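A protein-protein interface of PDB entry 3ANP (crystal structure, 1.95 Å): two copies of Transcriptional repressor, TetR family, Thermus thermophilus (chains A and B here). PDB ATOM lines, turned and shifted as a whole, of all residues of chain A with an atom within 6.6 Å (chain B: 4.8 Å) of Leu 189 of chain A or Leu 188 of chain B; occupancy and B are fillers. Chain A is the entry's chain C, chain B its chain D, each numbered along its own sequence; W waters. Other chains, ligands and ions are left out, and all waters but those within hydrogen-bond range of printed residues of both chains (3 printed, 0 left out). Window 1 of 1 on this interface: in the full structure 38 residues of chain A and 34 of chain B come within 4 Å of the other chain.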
ATOM      1  N   ARG A 146      25.095  23.177 -25.647  1.00  0.00           N
ATOM      2  CA  ARG A 146      25.745  21.997 -26.234  1.00  0.00           C
ATOM      3  C   ARG A 146      25.002  21.554 -27.498  1.00  0.00           C
ATOM      4  O   ARG A 146      23.799  21.792 -27.641  1.00  0.00           O
ATOM      5  CB  ARG A 146      25.788  20.850 -25.224  1.00  0.00           C
ATOM      6  CG  ARG A 146      24.417  20.316 -24.822  1.00  0.00           C
ATOM      7  CD  ARG A 146      24.558  19.440 -23.598  1.00  0.00           C
ATOM      8  NE  ARG A 146      25.522  18.373 -23.808  1.00  0.00           N
ATOM      9  CZ  ARG A 146      26.152  17.744 -22.827  1.00  0.00           C
ATOM     10  NH1 ARG A 146      25.911  18.082 -21.565  1.00  0.00           N
ATOM     11  NH2 ARG A 146      27.031  16.787 -23.105  1.00  0.00           N
ATOM     12  N   ASP A 148      25.527  18.218 -28.858  1.00  0.00           N
ATOM     13  CA  ASP A 148      25.578  16.766 -28.988  1.00  0.00           C
ATOM     14  C   ASP A 148      24.215  16.120 -28.738  1.00  0.00           C
ATOM     15  O   ASP A 148      24.090  14.898 -28.800  1.00  0.00           O
ATOM     16  CB  ASP A 148      26.646  16.170 -28.056  1.00  0.00           C
ATOM     17  CG  ASP A 148      26.530  16.661 -26.618  1.00  0.00           C
ATOM     18  OD1 ASP A 148      25.705  17.557 -26.342  1.00  0.00           O
ATOM     19  OD2 ASP A 148      27.278  16.150 -25.761  1.00  0.00           O
ATOM     20  N   PHE A 149      23.207  16.954 -28.456  1.00  0.00           N
ATOM     21  CA  PHE A 149      21.820  16.513 -28.246  1.00  0.00           C
ATOM     22  C   PHE A 149      20.929  17.518 -28.985  1.00  0.00           C
ATOM     23  O   PHE A 149      21.252  18.700 -29.040  1.00  0.00           O
ATOM     24  CB  PHE A 149      21.457  16.497 -26.753  1.00  0.00           C
ATOM     25  CG  PHE A 149      22.150  15.424 -25.976  1.00  0.00           C
ATOM     26  CD1 PHE A 149      21.903  14.078 -26.249  1.00  0.00           C
ATOM     27  CD2 PHE A 149      23.076  15.750 -24.988  1.00  0.00           C
ATOM     28  CE1 PHE A 149      22.569  13.069 -25.553  1.00  0.00           C
ATOM     29  CE2 PHE A 149      23.752  14.749 -24.279  1.00  0.00           C
ATOM     30  CZ  PHE A 149      23.498  13.405 -24.563  1.00  0.00           C
ATOM     31  N   ARG A 153      15.166  17.186 -28.018  1.00  0.00           N
ATOM     32  CA  ARG A 153      15.379  16.190 -26.987  1.00  0.00           C
ATOM     33  C   ARG A 153      15.628  16.837 -25.613  1.00  0.00           C
ATOM     34  O   ARG A 153      15.150  16.350 -24.588  1.00  0.00           O
ATOM     35  CB  ARG A 153      16.541  15.279 -27.380  1.00  0.00           C
ATOM     36  CG  ARG A 153      16.487  13.963 -26.679  1.00  0.00           C
ATOM     37  CD  ARG A 153      17.384  12.923 -27.332  1.00  0.00           C
ATOM     38  NE  ARG A 153      17.373  11.708 -26.531  1.00  0.00           N
ATOM     39  CZ  ARG A 153      18.402  10.875 -26.445  1.00  0.00           C
ATOM     40  NH1 ARG A 153      19.522  11.126 -27.120  1.00  0.00           N
ATOM     41  NH2 ARG A 153      18.319   9.809 -25.667  1.00  0.00           N
ATOM     42  N   MET A 154      16.373  17.931 -25.592  1.00  0.00           N
ATOM     43  CA  MET A 154      16.635  18.620 -24.333  1.00  0.00           C
ATOM     44  C   MET A 154      15.357  19.313 -23.863  1.00  0.00           C
ATOM     45  O   MET A 154      15.062  19.352 -22.668  1.00  0.00           O
ATOM     46  CB  MET A 154      17.779  19.622 -24.521  1.00  0.00           C
ATOM     47  CG  MET A 154      19.078  18.905 -24.912  1.00  0.00           C
ATOM     48  SD  MET A 154      20.651  20.016 -24.872  1.00  0.00           S
ATOM     49  CE  MET A 154      20.306  21.081 -26.445  1.00  0.00           C
ATOM     50  N   GLY A 155      14.602  19.850 -24.815  1.00  0.00           N
ATOM     51  CA  GLY A 155      13.338  20.494 -24.493  1.00  0.00           C
ATOM     52  C   GLY A 155      12.381  19.459 -23.914  1.00  0.00           C
ATOM     53  O   GLY A 155      11.693  19.729 -22.931  1.00  0.00           O
ATOM     54  N   THR A 157      13.111  16.735 -22.307  1.00  0.00           N
ATOM     55  CA  THR A 157      13.572  16.390 -20.973  1.00  0.00           C
ATOM     56  C   THR A 157      13.126  17.401 -19.923  1.00  0.00           C
ATOM     57  O   THR A 157      12.652  17.023 -18.840  1.00  0.00           O
ATOM     58  CB  THR A 157      15.126  16.262 -20.940  1.00  0.00           C
ATOM     59  OG1 THR A 157      15.535  15.178 -21.788  1.00  0.00           O
ATOM     60  CG2 THR A 157      15.614  15.997 -19.521  1.00  0.00           C
ATOM     61  N   LEU A 158      13.268  18.683 -20.230  1.00  0.00           N
ATOM     62  CA  LEU A 158      12.875  19.693 -19.274  1.00  0.00           C
ATOM     63  C   LEU A 158      11.364  19.670 -19.093  1.00  0.00           C
ATOM     64  O   LEU A 158      10.875  19.812 -17.969  1.00  0.00           O
ATOM     65  CB  LEU A 158      13.358  21.077 -19.711  1.00  0.00           C
ATOM     66  CG  LEU A 158      13.243  22.154 -18.625  1.00  0.00           C
ATOM     67  CD1 LEU A 158      13.871  21.651 -17.320  1.00  0.00           C
ATOM     68  CD2 LEU A 158      13.925  23.431 -19.103  1.00  0.00           C
ATOM     69  N   ALA A 159      10.618  19.468 -20.177  1.00  0.00           N
ATOM     70  CA  ALA A 159       9.154  19.390 -20.061  1.00  0.00           C
ATOM     71  C   ALA A 159       8.734  18.157 -19.257  1.00  0.00           C
ATOM     72  O   ALA A 159       7.748  18.191 -18.522  1.00  0.00           O
ATOM     73  CB  ALA A 159       8.505  19.351 -21.446  1.00  0.00           C
ATOM     74  N   LEU A 161      10.328  16.858 -16.771  1.00  0.00           N
ATOM     75  CA  LEU A 161      10.570  17.212 -15.371  1.00  0.00           C
ATOM     76  C   LEU A 161       9.458  18.111 -14.855  1.00  0.00           C
ATOM     77  O   LEU A 161       9.023  17.948 -13.720  1.00  0.00           O
ATOM     78  CB  LEU A 161      11.900  17.949 -15.190  1.00  0.00           C
ATOM     79  CG  LEU A 161      13.144  17.076 -15.069  1.00  0.00           C
ATOM     80  CD1 LEU A 161      14.340  17.955 -14.723  1.00  0.00           C
ATOM     81  CD2 LEU A 161      12.931  16.043 -13.977  1.00  0.00           C
ATOM     82  N   LYS A 184      14.283  24.882  -9.655  1.00  0.00           N
ATOM     83  CA  LYS A 184      15.323  23.891  -9.355  1.00  0.00           C
ATOM     84  C   LYS A 184      15.549  23.000 -10.580  1.00  0.00           C
ATOM     85  O   LYS A 184      16.694  22.727 -10.949  1.00  0.00           O
ATOM     86  CB  LYS A 184      14.919  23.015  -8.144  1.00  0.00           C
ATOM     87  CG  LYS A 184      15.861  21.813  -7.861  1.00  0.00           C
ATOM     88  CD  LYS A 184      15.420  20.500  -8.553  1.00  0.00           C
ATOM     89  CE  LYS A 184      14.082  20.007  -7.981  1.00  0.00           C
ATOM     90  NZ  LYS A 184      13.548  18.773  -8.632  1.00  0.00           N
ATOM     91  N   ASN A 185      14.463  22.542 -11.206  1.00  0.00           N
ATOM     92  CA  ASN A 185      14.580  21.694 -12.402  1.00  0.00           C
ATOM     93  C   ASN A 185      15.309  22.433 -13.507  1.00  0.00           C
ATOM     94  O   ASN A 185      16.178  21.876 -14.197  1.00  0.00           O
ATOM     95  CB  ASN A 185      13.201  21.289 -12.946  1.00  0.00           C
ATOM     96  CG  ASN A 185      12.452  20.363 -12.020  1.00  0.00           C
ATOM     97  OD1 ASN A 185      13.052  19.703 -11.179  1.00  0.00           O
ATOM     98  ND2 ASN A 185      11.128  20.289 -12.186  1.00  0.00           N
ATOM     99  N   LEU A 186      14.923  23.688 -13.701  1.00  0.00           N
ATOM    100  CA  LEU A 186      15.532  24.510 -14.724  1.00  0.00           C
ATOM    101  C   LEU A 186      17.034  24.702 -14.498  1.00  0.00           C
ATOM    102  O   LEU A 186      17.835  24.456 -15.392  1.00  0.00           O
ATOM    103  CB  LEU A 186      14.845  25.868 -14.771  1.00  0.00           C
ATOM    104  CG  LEU A 186      15.457  26.846 -15.771  1.00  0.00           C
ATOM    105  CD1 LEU A 186      15.340  26.274 -17.186  1.00  0.00           C
ATOM    106  CD2 LEU A 186      14.739  28.184 -15.671  1.00  0.00           C
ATOM    107  N   ARG A 187      17.407  25.157 -13.306  1.00  0.00           N
ATOM    108  CA  ARG A 187      18.812  25.379 -12.981  1.00  0.00           C
ATOM    109  C   ARG A 187      19.632  24.095 -13.133  1.00  0.00           C
ATOM    110  O   ARG A 187      20.720  24.101 -13.715  1.00  0.00           O
ATOM    111  CB  ARG A 187      18.949  25.873 -11.538  1.00  0.00           C
ATOM    112  CG  ARG A 187      18.111  27.093 -11.200  1.00  0.00           C
ATOM    113  CD  ARG A 187      18.815  28.381 -11.556  1.00  0.00           C
ATOM    114  NE  ARG A 187      20.138  28.455 -10.943  1.00  0.00           N
ATOM    115  CZ  ARG A 187      20.885  29.553 -10.908  1.00  0.00           C
ATOM    116  NH1 ARG A 187      20.437  30.679 -11.448  1.00  0.00           N
ATOM    117  NH2 ARG A 187      22.085  29.521 -10.345  1.00  0.00           N
ATOM    118  N   LEU A 188      19.128  22.995 -12.588  1.00  0.00           N
ATOM    119  CA  LEU A 188      19.866  21.743 -12.677  1.00  0.00           C
ATOM    120  C   LEU A 188      20.074  21.274 -14.105  1.00  0.00           C
ATOM    121  O   LEU A 188      21.198  20.924 -14.477  1.00  0.00           O
ATOM    122  CB  LEU A 188      19.191  20.635 -11.857  1.00  0.00           C
ATOM    123  CG  LEU A 188      19.370  20.734 -10.340  1.00  0.00           C
ATOM    124  CD1 LEU A 188      18.817  19.474  -9.687  1.00  0.00           C
ATOM    125  CD2 LEU A 188      20.860  20.884 -10.002  1.00  0.00           C
ATOM    126  N   LEU A 189      19.020  21.272 -14.924  1.00  0.00           N
ATOM    127  CA  LEU A 189      19.203  20.814 -16.295  1.00  0.00           C
ATOM    128  C   LEU A 189      19.956  21.827 -17.153  1.00  0.00           C
ATOM    129  O   LEU A 189      20.774  21.454 -17.995  1.00  0.00           O
ATOM    130  CB  LEU A 189      17.864  20.489 -16.964  1.00  0.00           C
ATOM    131  CG  LEU A 189      18.011  19.529 -18.151  1.00  0.00           C
ATOM    132  CD1 LEU A 189      18.218  18.109 -17.599  1.00  0.00           C
ATOM    133  CD2 LEU A 189      16.769  19.566 -19.059  1.00  0.00           C
ATOM    134  N   LEU A 190      19.690  23.112 -16.953  1.00  0.00           N
ATOM    135  CA  LEU A 190      20.379  24.120 -17.752  1.00  0.00           C
ATOM    136  C   LEU A 190      21.866  24.245 -17.388  1.00  0.00           C
ATOM    137  O   LEU A 190      22.730  24.202 -18.272  1.00  0.00           O
ATOM    138  CB  LEU A 190      19.694  25.479 -17.594  1.00  0.00           C
ATOM    139  CG  LEU A 190      20.205  26.655 -18.441  1.00  0.00           C
ATOM    140  CD1 LEU A 190      19.953  26.374 -19.909  1.00  0.00           C
ATOM    141  CD2 LEU A 190      19.478  27.945 -18.036  1.00  0.00           C
ATOM    142  N   GLU A 191      22.166  24.387 -16.095  1.00  0.00           N
ATOM    143  CA  GLU A 191      23.557  24.549 -15.650  1.00  0.00           C
ATOM    144  C   GLU A 191      24.273  23.264 -15.263  1.00  0.00           C
ATOM    145  O   GLU A 191      25.500  23.172 -15.390  1.00  0.00           O
ATOM    146  CB  GLU A 191      23.617  25.496 -14.449  1.00  0.00           C
ATOM    147  CG  GLU A 191      22.986  26.850 -14.704  1.00  0.00           C
ATOM    148  CD  GLU A 191      22.945  27.700 -13.443  1.00  0.00           C
ATOM    149  OE1 GLU A 191      22.510  27.185 -12.390  1.00  0.00           O
ATOM    150  OE2 GLU A 191      23.342  28.883 -13.506  1.00  0.00           O
ATOM    151  N   GLY A 192      23.513  22.281 -14.784  1.00  0.00           N
ATOM    152  CA  GLY A 192      24.113  21.032 -14.347  1.00  0.00           C
ATOM    153  C   GLY A 192      24.468  21.090 -12.865  1.00  0.00           C
ATOM    154  O   GLY A 192      24.446  22.168 -12.253  1.00  0.00           O
ATOM    155  N   MET A 193      24.784  19.936 -12.281  1.00  0.00           N
ATOM    156  CA  MET A 193      25.168  19.858 -10.865  1.00  0.00           C
ATOM    157  C   MET A 193      26.604  20.340 -10.668  1.00  0.00           C
ATOM    158  O   MET A 193      26.952  20.846  -9.599  1.00  0.00           O
ATOM    159  CB  MET A 193      25.082  18.407 -10.363  1.00  0.00           C
ATOM    160  CG  MET A 193      23.723  17.757 -10.570  1.00  0.00           C
ATOM    161  SD  MET A 193      23.805  15.908  -9.966  1.00  0.00           S
ATOM    162  CE  MET A 193      23.738  15.031 -11.685  1.00  0.00           C
ATOM    163  N   LEU B 161      14.352  11.337 -13.553  1.00  0.00           N
ATOM    164  CA  LEU B 161      14.585  11.237 -14.991  1.00  0.00           C
ATOM    165  C   LEU B 161      14.634   9.764 -15.396  1.00  0.00           C
ATOM    166  O   LEU B 161      14.140   9.387 -16.458  1.00  0.00           O
ATOM    167  CB  LEU B 161      15.897  11.954 -15.383  1.00  0.00           C
ATOM    168  CG  LEU B 161      15.826  13.493 -15.309  1.00  0.00           C
ATOM    169  CD1 LEU B 161      17.165  14.106 -15.690  1.00  0.00           C
ATOM    170  CD2 LEU B 161      14.728  14.011 -16.228  1.00  0.00           C
ATOM    171  N   LYS B 184      22.056   9.963 -21.543  1.00  0.00           N
ATOM    172  CA  LYS B 184      21.663  11.333 -21.879  1.00  0.00           C
ATOM    173  C   LYS B 184      21.183  12.044 -20.600  1.00  0.00           C
ATOM    174  O   LYS B 184      21.565  13.178 -20.331  1.00  0.00           O
ATOM    175  CB  LYS B 184      20.531  11.345 -22.913  1.00  0.00           C
ATOM    176  CG  LYS B 184      19.986  12.739 -23.201  1.00  0.00           C
ATOM    177  CD  LYS B 184      18.464  12.750 -23.264  1.00  0.00           C
ATOM    178  CE  LYS B 184      17.840  12.576 -21.906  1.00  0.00           C
ATOM    179  NZ  LYS B 184      16.368  12.261 -21.977  1.00  0.00           N
ATOM    180  N   ASN B 185      20.340  11.385 -19.811  1.00  0.00           N
ATOM    181  CA  ASN B 185      19.863  12.008 -18.575  1.00  0.00           C
ATOM    182  C   ASN B 185      21.068  12.371 -17.696  1.00  0.00           C
ATOM    183  O   ASN B 185      21.189  13.497 -17.204  1.00  0.00           O
ATOM    184  CB  ASN B 185      18.960  11.050 -17.794  1.00  0.00           C
ATOM    185  CG  ASN B 185      17.638  10.796 -18.483  1.00  0.00           C
ATOM    186  OD1 ASN B 185      17.246  11.522 -19.400  1.00  0.00           O
ATOM    187  ND2 ASN B 185      16.935   9.759 -18.036  1.00  0.00           N
ATOM    188  N   LEU B 186      21.956  11.401 -17.492  1.00  0.00           N
ATOM    189  CA  LEU B 186      23.147  11.626 -16.679  1.00  0.00           C
ATOM    190  C   LEU B 186      23.984  12.798 -17.191  1.00  0.00           C
ATOM    191  O   LEU B 186      24.355  13.667 -16.407  1.00  0.00           O
ATOM    192  CB  LEU B 186      24.012  10.362 -16.633  1.00  0.00           C
ATOM    193  CG  LEU B 186      25.354  10.489 -15.905  1.00  0.00           C
ATOM    194  CD1 LEU B 186      25.129  10.977 -14.473  1.00  0.00           C
ATOM    195  CD2 LEU B 186      26.044   9.127 -15.891  1.00  0.00           C
ATOM    196  N   ARG B 187      24.281  12.819 -18.493  1.00  0.00           N
ATOM    197  CA  ARG B 187      25.093  13.894 -19.088  1.00  0.00           C
ATOM    198  C   ARG B 187      24.467  15.267 -18.860  1.00  0.00           C
ATOM    199  O   ARG B 187      25.143  16.208 -18.415  1.00  0.00           O
ATOM    200  CB  ARG B 187      25.269  13.690 -20.602  1.00  0.00           C
ATOM    201  CG  ARG B 187      25.906  12.366 -21.013  1.00  0.00           C
ATOM    202  CD  ARG B 187      27.335  12.234 -20.515  1.00  0.00           C
ATOM    203  NE  ARG B 187      28.212  13.241 -21.108  1.00  0.00           N
ATOM    204  CZ  ARG B 187      28.431  13.372 -22.414  1.00  0.00           C
ATOM    205  NH1 ARG B 187      27.838  12.553 -23.277  1.00  0.00           N
ATOM    206  NH2 ARG B 187      29.238  14.329 -22.857  1.00  0.00           N
ATOM    207  N   LEU B 188      23.177  15.382 -19.168  1.00  0.00           N
ATOM    208  CA  LEU B 188      22.481  16.654 -19.008  1.00  0.00           C
ATOM    209  C   LEU B 188      22.364  17.132 -17.565  1.00  0.00           C
ATOM    210  O   LEU B 188      22.600  18.305 -17.267  1.00  0.00           O
ATOM    211  CB  LEU B 188      21.086  16.588 -19.640  1.00  0.00           C
ATOM    212  CG  LEU B 188      21.019  16.401 -21.162  1.00  0.00           C
ATOM    213  CD1 LEU B 188      19.567  16.467 -21.599  1.00  0.00           C
ATOM    214  CD2 LEU B 188      21.821  17.477 -21.878  1.00  0.00           C
ATOM    215  N   LEU B 189      22.011  16.247 -16.648  1.00  0.00           N
ATOM    216  CA  LEU B 189      21.887  16.717 -15.281  1.00  0.00           C
ATOM    217  C   LEU B 189      23.250  16.982 -14.642  1.00  0.00           C
ATOM    218  O   LEU B 189      23.411  17.946 -13.892  1.00  0.00           O
ATOM    219  CB  LEU B 189      21.100  15.726 -14.428  1.00  0.00           C
ATOM    220  CG  LEU B 189      20.472  16.421 -13.217  1.00  0.00           C
ATOM    221  CD1 LEU B 189      19.324  17.330 -13.710  1.00  0.00           C
ATOM    222  CD2 LEU B 189      19.954  15.393 -12.230  1.00  0.00           C
ATOM    223  N   LEU B 190      24.243  16.155 -14.951  1.00  0.00           N
ATOM    224  CA  LEU B 190      25.562  16.361 -14.353  1.00  0.00           C
ATOM    225  C   LEU B 190      26.270  17.593 -14.909  1.00  0.00           C
ATOM    226  O   LEU B 190      26.747  18.459 -14.157  1.00  0.00           O
ATOM    227  CB  LEU B 190      26.463  15.132 -14.580  1.00  0.00           C
ATOM    228  CG  LEU B 190      27.873  15.213 -13.978  1.00  0.00           C
ATOM    229  CD1 LEU B 190      27.792  15.323 -12.470  1.00  0.00           C
ATOM    230  CD2 LEU B 190      28.655  13.956 -14.353  1.00  0.00           C
ATOM    231  N   GLU B 191      26.319  17.666 -16.235  1.00  0.00           N
ATOM    232  CA  GLU B 191      27.017  18.737 -16.939  1.00  0.00           C
ATOM    233  C   GLU B 191      26.196  19.953 -17.314  1.00  0.00           C
ATOM    234  O   GLU B 191      26.732  21.056 -17.426  1.00  0.00           O
ATOM    235  CB  GLU B 191      27.635  18.178 -18.216  1.00  0.00           C
ATOM    236  CG  GLU B 191      28.617  17.048 -17.992  1.00  0.00           C
ATOM    237  CD  GLU B 191      28.800  16.224 -19.247  1.00  0.00           C
ATOM    238  OE1 GLU B 191      28.510  16.753 -20.343  1.00  0.00           O
ATOM    239  OE2 GLU B 191      29.235  15.058 -19.135  1.00  0.00           O
ATOM    240  N   GLY B 192      24.904  19.754 -17.511  1.00  0.00           N
ATOM    241  CA  GLY B 192      24.058  20.858 -17.907  1.00  0.00           C
ATOM    242  C   GLY B 192      24.012  20.988 -19.418  1.00  0.00           C
ATOM    243  O   GLY B 192      24.848  20.430 -20.145  1.00  0.00           O
ATOM    244  N   MET B 193      23.014  21.731 -19.888  1.00  0.00           N
ATOM    245  CA  MET B 193      22.818  21.976 -21.299  1.00  0.00           C
ATOM    246  C   MET B 193      23.790  23.028 -21.810  1.00  0.00           C
ATOM    247  O   MET B 193      24.180  22.986 -22.966  1.00  0.00           O
ATOM    248  CB  MET B 193      21.378  22.430 -21.549  1.00  0.00           C
ATOM    249  CG  MET B 193      20.366  21.341 -21.252  1.00  0.00           C
ATOM    250  SD  MET B 193      18.587  21.988 -21.667  1.00  0.00           S
ATOM    251  CE  MET B 193      19.045  23.075 -23.186  1.00  0.00           C
HETATM  252  O   HOH W   1      27.545  20.838 -20.752  1.00  0.00           O
HETATM  253  O   HOH W   2      14.092  13.398 -23.862  1.00  0.00           O
HETATM  254  O   HOH W   3      13.021  12.820 -21.302  1.00  0.00           O
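Of the printed residues of chain B, Asp 148 of chain A touches Arg 187.
Gly 155 of chain A touches none of the printed residues of chain B.
Of chain B, only Leu 188, Gly 192 and Met 193 come within 4 Å of Leu 189 of chain A.
Of the printed residues of chain B, Met 193 of chain A touches Leu 189 and Leu 190.
Of chain A, only Arg 146, Phe 149 and Leu 189 come within 4 Å of Leu 188 of chain B.
Printed residues of chain A that touch a printed residue of chain B: Arg 146, Asp 148, Phe 149, Arg 153, Met 154, Thr 157, Leu 161, Leu 188, Leu 189, Leu 190, Glu 191, Gly 192 and Met 193.
Of the 11 printed residues of chain B, 9 touch a printed residue of chain A.
Printed residues of chain B that touch a printed residue of chain A: Leu 161, Lys 184, Arg 187, Leu 188, Leu 189, Leu 190, Glu 191, Gly 192 and Met 193.
Along chain B the printed residues that touch a printed residue of chain A span positions 161 to 193.
Among the printed residues, 27 pairs touch across the chains.
NZ of Lys 184 of chain B sits close to OD1 of Asn 185 of chain B (2.8 Å).
NE of Arg 146 of chain A is in salt-bridge range of OD1 of Asp 148 of chain A (2.7 Å).
The backbone carbonyl oxygen (O) of Arg 153 of chain A sits at hydrogen-bond distance from the side-chain hydroxyl (OG1) of Thr 157 of chain A (3.1 Å).
NE of Arg 187 of chain B lies within salt-bridge range of OE2 of Glu 191 of chain B, at 2.9 Å.
The backbone carbonyl oxygen (O) of Leu 161 of chain B sits at hydrogen-bond distance from the side-chain amide nitrogen (ND2) of Asn 185 of chain B (3.2 Å).
The guanidinium group (NE) of Arg 187 of chain A lies within salt-bridge range of the side-chain carboxylate (OE1) of Glu 191 of chain A (3.1 Å).
The guanidinium group (NH2) of Arg 146 of chain A is in salt-bridge range of the side-chain carboxylate (OE1) of Glu 191 of chain B (3.1 Å).
The side-chain carboxylate of Asp 148 of chain A is in salt-bridge range of the guanidinium group of Arg 187 of chain B (3.9 Å).
O of Leu 189 of chain A is in hydrogen-bond range of N of Met 193 of chain B.
The backbone carbonyl oxygen (O) of Leu 190 of chain A is in hydrogen-bond range of the backbone NH (N) of Met 193 of chain B (3.0 Å).
The backbone NH of Arg 146 of chain A sits at hydrogen-bond distance from the backbone carbonyl oxygen of Met 193 of chain B.
The backbone carbonyl oxygen (O) of Glu 191 of chain A lies close to the backbone carbonyl oxygen (O) of Glu 191 of chain B.
The side-chain hydroxyl (OG1) of Thr 157 of chain A is in hydrogen-bond range of the side-chain amino group (NZ) of Lys 184 of chain B.
N of Met 193 of chain A sits at hydrogen-bond distance from O of Leu 189 of chain B, 2.9 Å away.
The guanidinium group (NH1) of Arg 146 of chain A sits at hydrogen-bond distance from the backbone carbonyl oxygen (O) of Gly 192 of chain B, 2.9 Å away.
The guanidinium group (NH2) of Arg 146 of chain A lies close to the guanidinium group (NH2) of Arg 187 of chain B (3.3 Å).
O of Leu 190 of chain B lies within hydrogen-bond range of N of Met 193 of chain A, at 3.1 Å.
Lys 184 of chain B touches Phe 149 of chain A (CG to CE1, 3.5 Å).
CD2 of Leu 188 of chain B touches CD2 of Phe 149 of chain A (3.8 Å).
Arg 153 of chain A touches Lys 184 of chain B.
CB of Met 154 of chain A touches SD of Met 193 of chain B (3.8 Å).
Thr 157 of chain A touches Leu 161 of chain B.
O of Leu 188 of chain A touches O of Leu 189 of chain B, 3.8 Å away.
O of Leu 189 of chain A touches O of Leu 188 of chain B, at 3.7 Å.
Gly 192 of chain B touches Glu 191 of chain A.
CA of Gly 192 of chain A touches O of Leu 189 of chain B (3.2 Å).
CA of Gly 192 of chain A touches C of Glu 191 of chain B (3.8 Å).
Leu 189 of chain A touches Gly 192 of chain B, and with the chains exchanged Gly 192 of chain A touches Leu 189 of chain B.
Leu 190 of chain A touches Gly 192 of chain B, and with the chains exchanged Gly 192 of chain A touches Leu 190 of chain B.
Glu 191 of chain A touches its own counterpart, Glu 191 of chain B.
Gly 192 of chain A touches its own counterpart, Gly 192 of chain B.
Of the 27 pairs that touch across the chains among the printed residues, 15 have their exchanged pair printed and touching as well.
Water W1 lies within hydrogen-bond range of the backbone carbonyl oxygen of Gly 192 of chain B, the guanidinium group of Arg 146 of chain A and the backbone carbonyl oxygen of Glu 191 of chain B.
Water W2 lies within hydrogen-bond range of OG1 of Thr 157 of chain A (3.1 Å), NZ of Lys 184 of chain B (3.2 Å) and O of Arg 153 of chain A (3.2 Å).
Water W3 lies within hydrogen-bond range of the side-chain amino group of Lys 184 of chain B (3.5 Å) and the side-chain hydroxyl of Thr 157 of chain A (3.5 Å).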
